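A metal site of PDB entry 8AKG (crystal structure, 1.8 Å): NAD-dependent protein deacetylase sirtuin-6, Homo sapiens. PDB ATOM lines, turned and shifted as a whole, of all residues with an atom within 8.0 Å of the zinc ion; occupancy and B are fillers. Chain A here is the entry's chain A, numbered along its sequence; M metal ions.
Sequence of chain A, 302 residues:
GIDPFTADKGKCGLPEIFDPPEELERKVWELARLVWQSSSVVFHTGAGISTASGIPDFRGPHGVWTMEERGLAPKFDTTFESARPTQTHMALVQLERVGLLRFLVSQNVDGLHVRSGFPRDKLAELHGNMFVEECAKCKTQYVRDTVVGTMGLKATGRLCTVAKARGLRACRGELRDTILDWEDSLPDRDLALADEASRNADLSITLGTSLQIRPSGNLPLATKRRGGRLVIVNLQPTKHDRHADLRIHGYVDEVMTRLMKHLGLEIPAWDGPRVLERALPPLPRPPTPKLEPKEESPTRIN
O of Thr 140 is in hydrogen-bond range of N of Cys 135 (2.9 Å).
SG of Cys 135 sits close to N of Lys 137 (3.4 Å).
NZ of Lys 137 lies within hydrogen-bond range of O of Cys 171, 3.5 Å away.
The backbone NH (N) of Gly 173 sits close to the side-chain sulfur (SG) of Cys 171, at 3.6 Å.
The backbone NH (N) of Arg 172 is in hydrogen-bond range of the backbone carbonyl oxygen (O) of Cys 160, 3.2 Å away.
The side-chain sulfur of Cys 160 sits close to the backbone NH of Val 162.
The side-chain sulfur (SG) of Cys 160 sits close to the side-chain hydroxyl (OH) of Tyr 142, at 3.0 Å.
The side-chain sulfur of Cys 138 lies close to the side-chain hydroxyl of Thr 140 (3.2 Å).
Within 4 Å of the zinc ion: Cys 135, Cys 138, Cys 160 and Cys 171.
The zinc ion is bound by the side-chain sulfur of Cys 138, the side-chain sulfur of Cys 160, the side-chain sulfur of Cys 135 and the side-chain sulfur of Cys 171.
The zinc ion has four donor atoms within binding distance.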
ATOM      1  N   GLU A 134     -25.418  -5.496  17.063  1.00  0.00           N
ATOM      2  CA  GLU A 134     -24.909  -4.503  18.038  1.00  0.00           C
ATOM      3  C   GLU A 134     -25.383  -3.112  17.618  1.00  0.00           C
ATOM      4  O   GLU A 134     -25.337  -2.802  16.409  1.00  0.00           O
ATOM      5  CB  GLU A 134     -23.379  -4.611  18.094  1.00  0.00           C
ATOM      6  CG  GLU A 134     -22.734  -3.588  18.995  1.00  0.00           C
ATOM      7  CD  GLU A 134     -21.220  -3.624  18.947  1.00  0.00           C
ATOM      8  OE1 GLU A 134     -20.655  -4.738  19.061  1.00  0.00           O
ATOM      9  OE2 GLU A 134     -20.599  -2.560  18.784  1.00  0.00           O
ATOM     10  N   CYS A 135     -25.842  -2.321  18.593  1.00  0.00           N
ATOM     11  CA  CYS A 135     -26.311  -0.925  18.366  1.00  0.00           C
ATOM     12  C   CYS A 135     -25.081  -0.036  18.143  1.00  0.00           C
ATOM     13  O   CYS A 135     -24.223  -0.003  19.032  1.00  0.00           O
ATOM     14  CB  CYS A 135     -27.101  -0.425  19.558  1.00  0.00           C
ATOM     15  SG  CYS A 135     -27.627   1.308  19.437  1.00  0.00           S
ATOM     16  N   ALA A 136     -25.023   0.653  17.012  1.00  0.00           N
ATOM     17  CA  ALA A 136     -23.917   1.586  16.692  1.00  0.00           C
ATOM     18  C   ALA A 136     -23.845   2.690  17.760  1.00  0.00           C
ATOM     19  O   ALA A 136     -22.729   3.073  18.136  1.00  0.00           O
ATOM     20  CB  ALA A 136     -24.125   2.186  15.330  1.00  0.00           C
ATOM     21  N   LYS A 137     -24.990   3.170  18.246  1.00  0.00           N
ATOM     22  CA  LYS A 137     -25.035   4.321  19.189  1.00  0.00           C
ATOM     23  C   LYS A 137     -24.541   3.901  20.580  1.00  0.00           C
ATOM     24  O   LYS A 137     -23.656   4.599  21.098  1.00  0.00           O
ATOM     25  CB  LYS A 137     -26.433   4.916  19.307  1.00  0.00           C
ATOM     26  CG  LYS A 137     -26.911   5.670  18.069  1.00  0.00           C
ATOM     27  CD  LYS A 137     -28.228   6.386  18.312  1.00  0.00           C
ATOM     28  CE  LYS A 137     -28.715   7.167  17.120  1.00  0.00           C
ATOM     29  NZ  LYS A 137     -30.056   7.755  17.369  1.00  0.00           N
ATOM     30  N   CYS A 138     -25.106   2.843  21.176  1.00  0.00           N
ATOM     31  CA  CYS A 138     -24.828   2.515  22.600  1.00  0.00           C
ATOM     32  C   CYS A 138     -24.026   1.214  22.731  1.00  0.00           C
ATOM     33  O   CYS A 138     -23.716   0.862  23.880  1.00  0.00           O
ATOM     34  CB  CYS A 138     -26.109   2.458  23.411  1.00  0.00           C
ATOM     35  SG  CYS A 138     -27.168   1.019  23.100  1.00  0.00           S
ATOM     36  N   LYS A 139     -23.702   0.539  21.628  1.00  0.00           N
ATOM     37  CA  LYS A 139     -22.852  -0.683  21.635  1.00  0.00           C
ATOM     38  C   LYS A 139     -23.555  -1.800  22.417  1.00  0.00           C
ATOM     39  O   LYS A 139     -22.861  -2.766  22.810  1.00  0.00           O
ATOM     40  CB  LYS A 139     -21.472  -0.379  22.226  1.00  0.00           C
ATOM     41  CG  LYS A 139     -20.813   0.897  21.713  1.00  0.00           C
ATOM     42  CD  LYS A 139     -20.666   0.954  20.214  1.00  0.00           C
ATOM     43  CE  LYS A 139     -19.931   2.189  19.750  1.00  0.00           C
ATOM     44  NZ  LYS A 139     -19.941   2.323  18.268  1.00  0.00           N
ATOM     45  N   THR A 140     -24.872  -1.726  22.591  1.00  0.00           N
ATOM     46  CA  THR A 140     -25.629  -2.810  23.269  1.00  0.00           C
ATOM     47  C   THR A 140     -25.788  -3.958  22.277  1.00  0.00           C
ATOM     48  O   THR A 140     -26.186  -3.701  21.137  1.00  0.00           O
ATOM     49  CB  THR A 140     -26.970  -2.331  23.840  1.00  0.00           C
ATOM     50  OG1 THR A 140     -26.698  -1.530  24.995  1.00  0.00           O
ATOM     51  CG2 THR A 140     -27.877  -3.477  24.260  1.00  0.00           C
ATOM     52  N   GLN A 141     -25.484  -5.175  22.724  1.00  0.00           N
ATOM     53  CA  GLN A 141     -25.510  -6.382  21.866  1.00  0.00           C
ATOM     54  C   GLN A 141     -26.806  -7.132  22.129  1.00  0.00           C
ATOM     55  O   GLN A 141     -27.344  -7.072  23.263  1.00  0.00           O
ATOM     56  CB  GLN A 141     -24.229  -7.190  22.080  1.00  0.00           C
ATOM     57  CG  GLN A 141     -22.994  -6.535  21.465  1.00  0.00           C
ATOM     58  CD  GLN A 141     -21.766  -7.405  21.584  1.00  0.00           C
ATOM     59  OE1 GLN A 141     -21.680  -8.243  22.471  1.00  0.00           O
ATOM     60  NE2 GLN A 141     -20.822  -7.236  20.669  1.00  0.00           N
ATOM     61  N   TYR A 142     -27.352  -7.723  21.069  1.00  0.00           N
ATOM     62  CA  TYR A 142     -28.584  -8.545  21.088  1.00  0.00           C
ATOM     63  C   TYR A 142     -28.190  -9.918  20.552  1.00  0.00           C
ATOM     64  O   TYR A 142     -27.694  -9.965  19.410  1.00  0.00           O
ATOM     65  CB  TYR A 142     -29.688  -7.895  20.250  1.00  0.00           C
ATOM     66  CG  TYR A 142     -30.115  -6.537  20.732  1.00  0.00           C
ATOM     67  CD1 TYR A 142     -29.439  -5.384  20.345  1.00  0.00           C
ATOM     68  CD2 TYR A 142     -31.213  -6.394  21.565  1.00  0.00           C
ATOM     69  CE1 TYR A 142     -29.834  -4.139  20.798  1.00  0.00           C
ATOM     70  CE2 TYR A 142     -31.625  -5.151  22.013  1.00  0.00           C
ATOM     71  CZ  TYR A 142     -30.933  -4.022  21.641  1.00  0.00           C
ATOM     72  OH  TYR A 142     -31.357  -2.811  22.104  1.00  0.00           O
ATOM     73  N   LEU A 159     -33.801  -1.687  15.160  1.00  0.00           N
ATOM     74  CA  LEU A 159     -33.402  -0.501  15.974  1.00  0.00           C
ATOM     75  C   LEU A 159     -33.280  -0.907  17.430  1.00  0.00           C
ATOM     76  O   LEU A 159     -34.009  -1.831  17.888  1.00  0.00           O
ATOM     77  CB  LEU A 159     -34.425   0.626  15.794  1.00  0.00           C
ATOM     78  CG  LEU A 159     -34.556   1.201  14.374  1.00  0.00           C
ATOM     79  CD1 LEU A 159     -35.442   2.438  14.383  1.00  0.00           C
ATOM     80  CD2 LEU A 159     -33.200   1.536  13.767  1.00  0.00           C
ATOM     81  N   CYS A 160     -32.407  -0.213  18.158  1.00  0.00           N
ATOM     82  CA  CYS A 160     -32.118  -0.465  19.581  1.00  0.00           C
ATOM     83  C   CYS A 160     -33.390  -0.240  20.405  1.00  0.00           C
ATOM     84  O   CYS A 160     -34.079   0.758  20.142  1.00  0.00           O
ATOM     85  CB  CYS A 160     -31.016   0.451  20.073  1.00  0.00           C
ATOM     86  SG  CYS A 160     -30.322  -0.036  21.671  1.00  0.00           S
ATOM     87  N   THR A 161     -33.677  -1.160  21.330  1.00  0.00           N
ATOM     88  CA  THR A 161     -34.865  -1.114  22.223  1.00  0.00           C
ATOM     89  C   THR A 161     -34.453  -0.648  23.622  1.00  0.00           C
ATOM     90  O   THR A 161     -35.310  -0.684  24.525  1.00  0.00           O
ATOM     91  CB  THR A 161     -35.565  -2.485  22.258  1.00  0.00           C
ATOM     92  OG1 THR A 161     -34.628  -3.492  22.631  1.00  0.00           O
ATOM     93  CG2 THR A 161     -36.186  -2.851  20.932  1.00  0.00           C
ATOM     94  N   VAL A 162     -33.184  -0.250  23.817  1.00  0.00           N
ATOM     95  CA  VAL A 162     -32.702   0.181  25.170  1.00  0.00           C
ATOM     96  C   VAL A 162     -33.582   1.307  25.715  1.00  0.00           C
ATOM     97  O   VAL A 162     -33.806   2.293  24.976  1.00  0.00           O
ATOM     98  CB  VAL A 162     -31.210   0.565  25.153  1.00  0.00           C
ATOM     99  CG1 VAL A 162     -30.844   1.523  26.279  1.00  0.00           C
ATOM    100  CG2 VAL A 162     -30.329  -0.675  25.208  1.00  0.00           C
ATOM    101  N   ALA A 163     -34.029   1.171  26.968  1.00  0.00           N
ATOM    102  CA  ALA A 163     -35.033   2.053  27.626  1.00  0.00           C
ATOM    103  C   ALA A 163     -34.843   3.502  27.169  1.00  0.00           C
ATOM    104  O   ALA A 163     -33.750   4.044  27.430  1.00  0.00           O
ATOM    105  CB  ALA A 163     -34.906   1.945  29.132  1.00  0.00           C
ATOM    106  N   CYS A 171     -33.386   4.734  22.438  1.00  0.00           N
ATOM    107  CA  CYS A 171     -32.109   4.814  21.680  1.00  0.00           C
ATOM    108  C   CYS A 171     -32.415   4.781  20.184  1.00  0.00           C
ATOM    109  O   CYS A 171     -31.885   5.638  19.455  1.00  0.00           O
ATOM    110  CB  CYS A 171     -31.178   3.675  22.085  1.00  0.00           C
ATOM    111  SG  CYS A 171     -29.557   3.739  21.276  1.00  0.00           S
ATOM    112  N   ARG A 172     -33.253   3.828  19.751  1.00  0.00           N
ATOM    113  CA  ARG A 172     -33.654   3.638  18.334  1.00  0.00           C
ATOM    114  C   ARG A 172     -32.391   3.629  17.458  1.00  0.00           C
ATOM    115  O   ARG A 172     -32.521   3.827  16.235  1.00  0.00           O
ATOM    116  CB  ARG A 172     -34.649   4.726  17.899  1.00  0.00           C
ATOM    117  CG  ARG A 172     -35.913   4.793  18.732  1.00  0.00           C
ATOM    118  CD  ARG A 172     -37.190   5.034  17.941  1.00  0.00           C
ATOM    119  NE  ARG A 172     -37.000   5.866  16.753  1.00  0.00           N
ATOM    120  CZ  ARG A 172     -37.313   5.530  15.499  1.00  0.00           C
ATOM    121  NH1 ARG A 172     -37.871   4.364  15.222  1.00  0.00           N
ATOM    122  NH2 ARG A 172     -37.074   6.376  14.507  1.00  0.00           N
ATOM    123  N   GLY A 173     -31.227   3.381  18.066  1.00  0.00           N
ATOM    124  CA  GLY A 173     -29.946   3.236  17.359  1.00  0.00           C
ATOM    125  C   GLY A 173     -30.024   2.142  16.313  1.00  0.00           C
ATOM    126  O   GLY A 173     -30.762   1.161  16.525  1.00  0.00           O
ATOM    127  N   GLU A 174     -29.280   2.312  15.217  1.00  0.00           N
ATOM    128  CA  GLU A 174     -29.134   1.350  14.105  1.00  0.00           C
ATOM    129  C   GLU A 174     -28.430   0.078  14.627  1.00  0.00           C
ATOM    130  O   GLU A 174     -27.240   0.175  15.018  1.00  0.00           O
ATOM    131  CB  GLU A 174     -28.330   2.027  12.992  1.00  0.00           C
ATOM    132  CG  GLU A 174     -28.329   1.306  11.651  1.00  0.00           C
ATOM    133  CD  GLU A 174     -27.660   2.110  10.545  1.00  0.00           C
ATOM    134  OE1 GLU A 174     -28.092   3.253  10.321  1.00  0.00           O
ATOM    135  OE2 GLU A 174     -26.700   1.598   9.929  1.00  0.00           O
ATOM    136  N   LEU A 175     -29.113  -1.072  14.624  1.00  0.00           N
ATOM    137  CA  LEU A 175     -28.442  -2.363  14.937  1.00  0.00           C
ATOM    138  C   LEU A 175     -27.721  -2.845  13.679  1.00  0.00           C
ATOM    139  O   LEU A 175     -28.355  -2.809  12.612  1.00  0.00           O
ATOM    140  CB  LEU A 175     -29.435  -3.436  15.383  1.00  0.00           C
ATOM    141  CG  LEU A 175     -30.307  -3.079  16.579  1.00  0.00           C
ATOM    142  CD1 LEU A 175     -31.118  -4.300  17.004  1.00  0.00           C
ATOM    143  CD2 LEU A 175     -29.466  -2.551  17.731  1.00  0.00           C
HETATM  144 ZN    ZN M   1     -28.663   1.529  21.508  1.00  0.00          ZN
